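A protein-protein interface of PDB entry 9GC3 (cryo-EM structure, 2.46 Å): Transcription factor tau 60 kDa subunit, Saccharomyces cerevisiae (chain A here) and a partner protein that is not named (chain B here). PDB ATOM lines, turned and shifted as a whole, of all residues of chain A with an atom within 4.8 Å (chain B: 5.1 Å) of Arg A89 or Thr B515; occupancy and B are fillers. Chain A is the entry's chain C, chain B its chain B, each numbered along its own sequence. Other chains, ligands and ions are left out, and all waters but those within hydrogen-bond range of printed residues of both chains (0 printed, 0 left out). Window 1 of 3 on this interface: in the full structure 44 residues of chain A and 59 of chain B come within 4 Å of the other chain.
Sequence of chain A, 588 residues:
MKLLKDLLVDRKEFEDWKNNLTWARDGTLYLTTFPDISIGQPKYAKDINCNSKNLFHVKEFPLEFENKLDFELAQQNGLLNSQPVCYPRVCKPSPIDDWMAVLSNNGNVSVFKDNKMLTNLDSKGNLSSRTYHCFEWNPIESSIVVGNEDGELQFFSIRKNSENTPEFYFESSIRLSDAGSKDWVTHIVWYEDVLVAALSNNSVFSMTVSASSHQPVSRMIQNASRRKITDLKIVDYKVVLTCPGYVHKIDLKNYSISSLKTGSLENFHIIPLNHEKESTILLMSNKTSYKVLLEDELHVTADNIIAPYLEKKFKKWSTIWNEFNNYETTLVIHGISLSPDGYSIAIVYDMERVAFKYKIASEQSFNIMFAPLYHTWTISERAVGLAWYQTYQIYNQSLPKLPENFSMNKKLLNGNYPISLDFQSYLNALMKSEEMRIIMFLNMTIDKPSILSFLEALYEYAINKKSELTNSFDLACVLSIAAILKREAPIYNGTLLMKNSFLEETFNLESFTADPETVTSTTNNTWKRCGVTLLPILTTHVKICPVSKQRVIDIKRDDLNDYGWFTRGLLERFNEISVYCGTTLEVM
O of Thr B514 lies within hydrogen-bond range of NE of Arg A89, at 3.0 Å.
ND1 of His A133 is in hydrogen-bond range of OG1 of Thr B514 (2.8 Å).
NZ of Lys B516 sits at hydrogen-bond distance from O of Glu A15 (2.8 Å).
O of Lys B516 is in hydrogen-bond range of NH1 of Arg A89 (2.7 Å).
The backbone NH (N) of Arg A89 lies within hydrogen-bond range of the backbone carbonyl oxygen (O) of Leu A103 (2.8 Å).
OD2 of Asp B511 is in hydrogen-bond range of OG1 of Thr B514 (3.0 Å).
The side-chain amide oxygen (OD1) of Asn A105 sits at hydrogen-bond distance from the backbone NH (N) of Tyr A87 (2.9 Å).
The side-chain hydroxyl (OG1) of Thr A32 sits at hydrogen-bond distance from the backbone carbonyl oxygen (O) of Arg A89 (3.3 Å).
O of Thr B515 lies within hydrogen-bond range of OG1 of Thr B517.
The side-chain amide oxygen (OD1) of Asn A20 sits at hydrogen-bond distance from the side-chain amino group (NZ) of Lys A18 (3.0 Å).
Among the printed residues, pairs that only touch across the chains: Lys A18 with Ala B513 (3.9 Å), Leu A79 with Ile B506 (3.7 Å), Leu A79 with Phe B507 (3.7 Å), Leu A79 with Asn B508 (3.6 Å), Leu A79 with Thr B515 (3.5 Å), Tyr A87 with Lys B516 (3.6 Å), Arg A89 with Ala B513 (3.3 Å), Arg A89 with Thr B515 (3.7 Å), Trp A184 with Asn B508 (3.6 Å) and Trp A184 with Thr B515 (3.6 Å).
Of the printed residues of chain B, Leu A79 touches Ile B506 (3.7 Å), Phe B507 (3.7 Å), Asn B508 (3.6 Å) and Thr B515 (3.5 Å).
Of the printed residues of chain B, Arg A89 touches Ala B513, Thr B514, Thr B515 and Lys B516.
Ile B512 touches none of the printed residues of chain A.
Of chain A, only Leu A79 (3.5 Å), Arg A89 (3.7 Å) and Trp A184 (3.6 Å) come within 4 Å of Thr B515.
Of the printed residues of chain A, Lys B516 touches Glu A15 (2.8 Å), Tyr A87 (3.6 Å) and Arg A89 (2.7 Å).
Thr B517 touches none of the printed residues of chain A.
The nearest printed residue of chain B that does not touch Tyr A87 is Thr B517 (5.0 Å).
Hydrophobic or aromatic side chains of chain B that line the printed part of chain A: Ile B506 and Ala B513.
Of the 16 printed residues of chain A, 7 touch a printed residue of chain B.
Among the printed residues, no Asp or Glu carboxylate lies within 4 Å of a Lys or Arg side-chain nitrogen of the other chain.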
ATOM      1  N   GLU A  15      22.266  -5.968   4.782  1.00  0.00           N
ATOM      2  CA  GLU A  15      23.707  -5.743   5.025  1.00  0.00           C
ATOM      3  C   GLU A  15      24.463  -6.042   3.733  1.00  0.00           C
ATOM      4  O   GLU A  15      25.510  -5.424   3.477  1.00  0.00           O
ATOM      5  CB  GLU A  15      24.232  -6.607   6.160  1.00  0.00           C
ATOM      6  CG  GLU A  15      25.706  -6.372   6.397  1.00  0.00           C
ATOM      7  CD  GLU A  15      26.270  -7.011   7.641  1.00  0.00           C
ATOM      8  OE1 GLU A  15      26.032  -8.224   7.828  1.00  0.00           O
ATOM      9  OE2 GLU A  15      26.941  -6.300   8.416  1.00  0.00           O
ATOM     10  N   LYS A  18      23.688 -10.901  -1.240  1.00  0.00           N
ATOM     11  CA  LYS A  18      23.347 -12.319  -1.476  1.00  0.00           C
ATOM     12  C   LYS A  18      21.834 -12.551  -1.404  1.00  0.00           C
ATOM     13  O   LYS A  18      21.025 -11.592  -1.297  1.00  0.00           O
ATOM     14  CB  LYS A  18      24.051 -13.149  -0.415  1.00  0.00           C
ATOM     15  CG  LYS A  18      23.404 -13.122   0.951  1.00  0.00           C
ATOM     16  CD  LYS A  18      24.349 -13.710   1.957  1.00  0.00           C
ATOM     17  CE  LYS A  18      23.705 -13.962   3.290  1.00  0.00           C
ATOM     18  NZ  LYS A  18      23.169 -12.721   3.896  1.00  0.00           N
ATOM     19  N   ASN A  20      18.700 -13.153   0.215  1.00  0.00           N
ATOM     20  CA  ASN A  20      18.197 -12.902   1.577  1.00  0.00           C
ATOM     21  C   ASN A  20      16.729 -13.297   1.733  1.00  0.00           C
ATOM     22  O   ASN A  20      16.152 -12.897   2.730  1.00  0.00           O
ATOM     23  CB  ASN A  20      18.373 -11.434   1.892  1.00  0.00           C
ATOM     24  CG  ASN A  20      19.819 -11.056   2.122  1.00  0.00           C
ATOM     25  OD1 ASN A  20      20.594 -11.807   2.713  1.00  0.00           O
ATOM     26  ND2 ASN A  20      20.185  -9.872   1.689  1.00  0.00           N
ATOM     27  N   THR A  32      16.116 -11.786   5.574  1.00  0.00           N
ATOM     28  CA  THR A  32      17.227 -11.526   6.525  1.00  0.00           C
ATOM     29  C   THR A  32      17.688 -10.097   6.268  1.00  0.00           C
ATOM     30  O   THR A  32      18.822  -9.864   5.939  1.00  0.00           O
ATOM     31  CB  THR A  32      18.276 -12.638   6.487  1.00  0.00           C
ATOM     32  OG1 THR A  32      19.296 -12.312   7.429  1.00  0.00           O
ATOM     33  CG2 THR A  32      18.856 -12.830   5.114  1.00  0.00           C
ATOM     34  N   ASN A  77      40.456 -17.265  12.325  1.00  0.00           N
ATOM     35  CA  ASN A  77      39.399 -16.368  11.814  1.00  0.00           C
ATOM     36  C   ASN A  77      39.329 -15.173  12.753  1.00  0.00           C
ATOM     37  O   ASN A  77      38.484 -15.171  13.680  1.00  0.00           O
ATOM     38  CB  ASN A  77      38.066 -17.078  11.684  1.00  0.00           C
ATOM     39  CG  ASN A  77      36.967 -16.202  11.128  1.00  0.00           C
ATOM     40  OD1 ASN A  77      37.228 -15.144  10.579  1.00  0.00           O
ATOM     41  ND2 ASN A  77      35.730 -16.618  11.293  1.00  0.00           N
ATOM     42  N   LEU A  79      38.013 -12.398  12.347  1.00  0.00           N
ATOM     43  CA  LEU A  79      36.718 -11.677  12.320  1.00  0.00           C
ATOM     44  C   LEU A  79      35.712 -12.304  13.285  1.00  0.00           C
ATOM     45  O   LEU A  79      34.708 -11.628  13.544  1.00  0.00           O
ATOM     46  CB  LEU A  79      36.214 -11.540  10.878  1.00  0.00           C
ATOM     47  CG  LEU A  79      37.097 -10.640  10.012  1.00  0.00           C
ATOM     48  CD1 LEU A  79      36.616 -10.577   8.575  1.00  0.00           C
ATOM     49  CD2 LEU A  79      37.187  -9.248  10.597  1.00  0.00           C
ATOM     50  N   TYR A  87      23.827 -10.621  15.319  1.00  0.00           N
ATOM     51  CA  TYR A  87      22.690 -10.326  14.436  1.00  0.00           C
ATOM     52  C   TYR A  87      22.639 -11.419  13.381  1.00  0.00           C
ATOM     53  O   TYR A  87      23.631 -12.093  13.123  1.00  0.00           O
ATOM     54  CB  TYR A  87      22.842  -8.921  13.861  1.00  0.00           C
ATOM     55  CG  TYR A  87      23.972  -8.761  12.885  1.00  0.00           C
ATOM     56  CD1 TYR A  87      23.861  -9.149  11.547  1.00  0.00           C
ATOM     57  CD2 TYR A  87      25.173  -8.229  13.319  1.00  0.00           C
ATOM     58  CE1 TYR A  87      24.935  -9.029  10.675  1.00  0.00           C
ATOM     59  CE2 TYR A  87      26.243  -8.086  12.454  1.00  0.00           C
ATOM     60  CZ  TYR A  87      26.123  -8.471  11.128  1.00  0.00           C
ATOM     61  OH  TYR A  87      27.224  -8.345  10.328  1.00  0.00           O
ATOM     62  N   PRO A  88      21.465 -11.643  12.780  1.00  0.00           N
ATOM     63  CA  PRO A  88      21.317 -12.734  11.830  1.00  0.00           C
ATOM     64  C   PRO A  88      21.971 -12.485  10.474  1.00  0.00           C
ATOM     65  O   PRO A  88      21.831 -11.439   9.928  1.00  0.00           O
ATOM     66  CB  PRO A  88      19.784 -12.877  11.718  1.00  0.00           C
ATOM     67  CG  PRO A  88      19.259 -11.516  12.010  1.00  0.00           C
ATOM     68  CD  PRO A  88      20.217 -10.913  13.019  1.00  0.00           C
ATOM     69  N   ARG A  89      22.638 -13.505   9.964  1.00  0.00           N
ATOM     70  CA  ARG A  89      23.183 -13.531   8.596  1.00  0.00           C
ATOM     71  C   ARG A  89      22.317 -14.386   7.681  1.00  0.00           C
ATOM     72  O   ARG A  89      22.066 -13.957   6.565  1.00  0.00           O
ATOM     73  CB  ARG A  89      24.592 -14.125   8.578  1.00  0.00           C
ATOM     74  CG  ARG A  89      25.664 -13.133   8.983  1.00  0.00           C
ATOM     75  CD  ARG A  89      26.965 -13.415   8.254  1.00  0.00           C
ATOM     76  NE  ARG A  89      28.081 -12.711   8.886  1.00  0.00           N
ATOM     77  CZ  ARG A  89      28.317 -11.435   8.727  1.00  0.00           C
ATOM     78  NH1 ARG A  89      29.326 -10.870   9.356  1.00  0.00           N
ATOM     79  NH2 ARG A  89      27.539 -10.713   7.946  1.00  0.00           N
ATOM     80  N   VAL A  90      21.997 -15.606   8.084  1.00  0.00           N
ATOM     81  CA  VAL A  90      21.234 -16.533   7.212  1.00  0.00           C
ATOM     82  C   VAL A  90      20.093 -17.118   8.036  1.00  0.00           C
ATOM     83  O   VAL A  90      20.299 -17.444   9.202  1.00  0.00           O
ATOM     84  CB  VAL A  90      22.163 -17.622   6.642  1.00  0.00           C
ATOM     85  CG1 VAL A  90      21.405 -18.629   5.792  1.00  0.00           C
ATOM     86  CG2 VAL A  90      23.315 -17.007   5.856  1.00  0.00           C
ATOM     87  N   CYS A  91      18.934 -17.256   7.426  1.00  0.00           N
ATOM     88  CA  CYS A  91      17.727 -17.802   8.067  1.00  0.00           C
ATOM     89  C   CYS A  91      17.131 -18.841   7.121  1.00  0.00           C
ATOM     90  O   CYS A  91      16.744 -18.463   5.989  1.00  0.00           O
ATOM     91  CB  CYS A  91      16.757 -16.674   8.388  1.00  0.00           C
ATOM     92  SG  CYS A  91      15.173 -17.294   8.980  1.00  0.00           S
ATOM     93  N   LEU A 103      21.760 -18.553  11.373  1.00  0.00           N
ATOM     94  CA  LEU A 103      23.213 -18.330  11.532  1.00  0.00           C
ATOM     95  C   LEU A 103      23.462 -16.869  11.921  1.00  0.00           C
ATOM     96  O   LEU A 103      23.040 -15.971  11.175  1.00  0.00           O
ATOM     97  CB  LEU A 103      23.889 -18.682  10.212  1.00  0.00           C
ATOM     98  CG  LEU A 103      25.381 -18.416  10.142  1.00  0.00           C
ATOM     99  CD1 LEU A 103      26.154 -19.346  11.056  1.00  0.00           C
ATOM    100  CD2 LEU A 103      25.872 -18.557   8.714  1.00  0.00           C
ATOM    101  N   SER A 104      24.120 -16.617  13.048  1.00  0.00           N
ATOM    102  CA  SER A 104      24.504 -15.238  13.438  1.00  0.00           C
ATOM    103  C   SER A 104      25.804 -14.822  12.725  1.00  0.00           C
ATOM    104  O   SER A 104      26.541 -15.666  12.148  1.00  0.00           O
ATOM    105  CB  SER A 104      24.624 -15.102  14.899  1.00  0.00           C
ATOM    106  OG  SER A 104      25.869 -15.635  15.363  1.00  0.00           O
ATOM    107  N   ASN A 105      26.086 -13.536  12.784  1.00  0.00           N
ATOM    108  CA  ASN A 105      27.350 -12.942  12.281  1.00  0.00           C
ATOM    109  C   ASN A 105      28.572 -13.557  13.000  1.00  0.00           C
ATOM    110  O   ASN A 105      29.669 -13.484  12.450  1.00  0.00           O
ATOM    111  CB  ASN A 105      27.306 -11.426  12.463  1.00  0.00           C
ATOM    112  CG  ASN A 105      27.195 -11.024  13.915  1.00  0.00           C
ATOM    113  OD1 ASN A 105      26.429 -11.608  14.673  1.00  0.00           O
ATOM    114  ND2 ASN A 105      27.956 -10.035  14.329  1.00  0.00           N
ATOM    115  N   HIS A 133      29.651 -21.713   9.385  1.00  0.00           N
ATOM    116  CA  HIS A 133      29.494 -20.783   8.244  1.00  0.00           C
ATOM    117  C   HIS A 133      28.355 -21.196   7.316  1.00  0.00           C
ATOM    118  O   HIS A 133      28.048 -20.430   6.384  1.00  0.00           O
ATOM    119  CB  HIS A 133      30.784 -20.694   7.444  1.00  0.00           C
ATOM    120  CG  HIS A 133      31.841 -19.927   8.161  1.00  0.00           C
ATOM    121  ND1 HIS A 133      31.943 -18.567   8.056  1.00  0.00           N
ATOM    122  CD2 HIS A 133      32.824 -20.325   8.999  1.00  0.00           C
ATOM    123  CE1 HIS A 133      32.958 -18.156   8.780  1.00  0.00           C
ATOM    124  NE2 HIS A 133      33.516 -19.214   9.365  1.00  0.00           N
ATOM    125  N   TRP A 184      37.076 -23.733   4.961  1.00  0.00           N
ATOM    126  CA  TRP A 184      35.756 -23.720   5.622  1.00  0.00           C
ATOM    127  C   TRP A 184      34.738 -24.386   4.722  1.00  0.00           C
ATOM    128  O   TRP A 184      34.897 -24.311   3.494  1.00  0.00           O
ATOM    129  CB  TRP A 184      35.317 -22.301   5.956  1.00  0.00           C
ATOM    130  CG  TRP A 184      36.336 -21.490   6.689  1.00  0.00           C
ATOM    131  CD1 TRP A 184      37.455 -21.924   7.337  1.00  0.00           C
ATOM    132  CD2 TRP A 184      36.289 -20.068   6.847  1.00  0.00           C
ATOM    133  NE1 TRP A 184      38.107 -20.863   7.890  1.00  0.00           N
ATOM    134  CE2 TRP A 184      37.417 -19.715   7.607  1.00  0.00           C
ATOM    135  CE3 TRP A 184      35.399 -19.063   6.435  1.00  0.00           C
ATOM    136  CZ2 TRP A 184      37.696 -18.389   7.933  1.00  0.00           C
ATOM    137  CZ3 TRP A 184      35.683 -17.754   6.748  1.00  0.00           C
ATOM    138  CH2 TRP A 184      36.815 -17.423   7.498  1.00  0.00           C
ATOM    139  N   ILE B 506      35.098  -4.633   6.869  1.00  0.00           N
ATOM    140  CA  ILE B 506      36.203  -5.628   6.850  1.00  0.00           C
ATOM    141  C   ILE B 506      35.572  -6.976   6.534  1.00  0.00           C
ATOM    142  O   ILE B 506      34.585  -7.347   7.192  1.00  0.00           O
ATOM    143  CB  ILE B 506      36.978  -5.639   8.184  1.00  0.00           C
ATOM    144  CG1 ILE B 506      37.531  -4.263   8.517  1.00  0.00           C
ATOM    145  CG2 ILE B 506      38.115  -6.657   8.124  1.00  0.00           C
ATOM    146  CD1 ILE B 506      38.194  -4.180   9.854  1.00  0.00           C
ATOM    147  N   PHE B 507      36.130  -7.712   5.598  1.00  0.00           N
ATOM    148  CA  PHE B 507      35.639  -9.069   5.290  1.00  0.00           C
ATOM    149  C   PHE B 507      36.834  -9.964   4.958  1.00  0.00           C
ATOM    150  O   PHE B 507      37.951  -9.481   4.661  1.00  0.00           O
ATOM    151  CB  PHE B 507      34.633  -9.045   4.130  1.00  0.00           C
ATOM    152  CG  PHE B 507      35.191  -8.451   2.869  1.00  0.00           C
ATOM    153  CD1 PHE B 507      35.825  -9.266   1.948  1.00  0.00           C
ATOM    154  CD2 PHE B 507      35.063  -7.092   2.580  1.00  0.00           C
ATOM    155  CE1 PHE B 507      36.347  -8.730   0.777  1.00  0.00           C
ATOM    156  CE2 PHE B 507      35.559  -6.565   1.397  1.00  0.00           C
ATOM    157  CZ  PHE B 507      36.219  -7.385   0.508  1.00  0.00           C
ATOM    158  N   ASN B 508      36.581 -11.268   5.006  1.00  0.00           N
ATOM    159  CA  ASN B 508      37.554 -12.287   4.585  1.00  0.00           C
ATOM    160  C   ASN B 508      37.208 -12.741   3.176  1.00  0.00           C
ATOM    161  O   ASN B 508      36.104 -13.209   2.943  1.00  0.00           O
ATOM    162  CB  ASN B 508      37.540 -13.454   5.548  1.00  0.00           C
ATOM    163  CG  ASN B 508      38.634 -14.449   5.246  1.00  0.00           C
ATOM    164  OD1 ASN B 508      38.958 -14.713   4.085  1.00  0.00           O
ATOM    165  ND2 ASN B 508      39.184 -15.016   6.292  1.00  0.00           N
ATOM    166  N   ASP B 511      35.089 -16.033   2.389  1.00  0.00           N
ATOM    167  CA  ASP B 511      33.610 -16.031   2.424  1.00  0.00           C
ATOM    168  C   ASP B 511      33.140 -14.649   2.865  1.00  0.00           C
ATOM    169  O   ASP B 511      32.990 -14.410   4.077  1.00  0.00           O
ATOM    170  CB  ASP B 511      33.065 -17.163   3.298  1.00  0.00           C
ATOM    171  CG  ASP B 511      31.633 -17.533   2.940  1.00  0.00           C
ATOM    172  OD1 ASP B 511      31.050 -16.860   2.057  1.00  0.00           O
ATOM    173  OD2 ASP B 511      31.108 -18.509   3.520  1.00  0.00           O
ATOM    174  N   ILE B 512      32.907 -13.777   1.893  1.00  0.00           N
ATOM    175  CA  ILE B 512      32.479 -12.379   2.154  1.00  0.00           C
ATOM    176  C   ILE B 512      31.136 -12.414   2.883  1.00  0.00           C
ATOM    177  O   ILE B 512      30.958 -11.635   3.861  1.00  0.00           O
ATOM    178  CB  ILE B 512      32.427 -11.559   0.853  1.00  0.00           C
ATOM    179  CG1 ILE B 512      33.770 -11.656   0.115  1.00  0.00           C
ATOM    180  CG2 ILE B 512      32.053 -10.114   1.173  1.00  0.00           C
ATOM    181  CD1 ILE B 512      33.942 -10.688  -1.026  1.00  0.00           C
ATOM    182  N   ALA B 513      30.250 -13.301   2.439  1.00  0.00           N
ATOM    183  CA  ALA B 513      28.871 -13.425   2.960  1.00  0.00           C
ATOM    184  C   ALA B 513      28.900 -13.656   4.477  1.00  0.00           C
ATOM    185  O   ALA B 513      28.193 -12.947   5.199  1.00  0.00           O
ATOM    186  CB  ALA B 513      28.150 -14.538   2.252  1.00  0.00           C
ATOM    187  N   THR B 514      29.736 -14.558   4.957  1.00  0.00           N
ATOM    188  CA  THR B 514      29.711 -14.953   6.381  1.00  0.00           C
ATOM    189  C   THR B 514      30.678 -14.131   7.209  1.00  0.00           C
ATOM    190  O   THR B 514      30.591 -14.250   8.453  1.00  0.00           O
ATOM    191  CB  THR B 514      30.001 -16.442   6.574  1.00  0.00           C
ATOM    192  OG1 THR B 514      31.276 -16.732   5.991  1.00  0.00           O
ATOM    193  CG2 THR B 514      28.903 -17.283   5.963  1.00  0.00           C
ATOM    194  N   THR B 515      31.549 -13.327   6.602  1.00  0.00           N
ATOM    195  CA  THR B 515      32.590 -12.593   7.388  1.00  0.00           C
ATOM    196  C   THR B 515      32.396 -11.079   7.377  1.00  0.00           C
ATOM    197  O   THR B 515      33.124 -10.423   8.116  1.00  0.00           O
ATOM    198  CB  THR B 515      33.974 -12.992   6.887  1.00  0.00           C
ATOM    199  OG1 THR B 515      34.126 -12.613   5.509  1.00  0.00           O
ATOM    200  CG2 THR B 515      34.164 -14.485   7.082  1.00  0.00           C
ATOM    201  N   LYS B 516      31.582 -10.536   6.477  1.00  0.00           N
ATOM    202  CA  LYS B 516      31.483  -9.061   6.315  1.00  0.00           C
ATOM    203  C   LYS B 516      31.135  -8.398   7.655  1.00  0.00           C
ATOM    204  O   LYS B 516      30.087  -8.610   8.188  1.00  0.00           O
ATOM    205  CB  LYS B 516      30.463  -8.741   5.240  1.00  0.00           C
ATOM    206  CG  LYS B 516      30.351  -7.289   4.850  1.00  0.00           C
ATOM    207  CD  LYS B 516      29.388  -7.144   3.701  1.00  0.00           C
ATOM    208  CE  LYS B 516      29.189  -5.723   3.252  1.00  0.00           C
ATOM    209  NZ  LYS B 516      28.042  -5.607   2.333  1.00  0.00           N
ATOM    210  N   THR B 517      32.012  -7.536   8.134  1.00  0.00           N
ATOM    211  CA  THR B 517      31.924  -6.851   9.439  1.00  0.00           C
ATOM    212  C   THR B 517      31.894  -5.346   9.199  1.00  0.00           C
ATOM    213  O   THR B 517      32.726  -4.829   8.474  1.00  0.00           O
ATOM    214  CB  THR B 517      33.136  -7.247  10.287  1.00  0.00           C
ATOM    215  OG1 THR B 517      33.148  -8.663  10.479  1.00  0.00           O
ATOM    216  CG2 THR B 517      33.142  -6.569  11.636  1.00  0.00           C
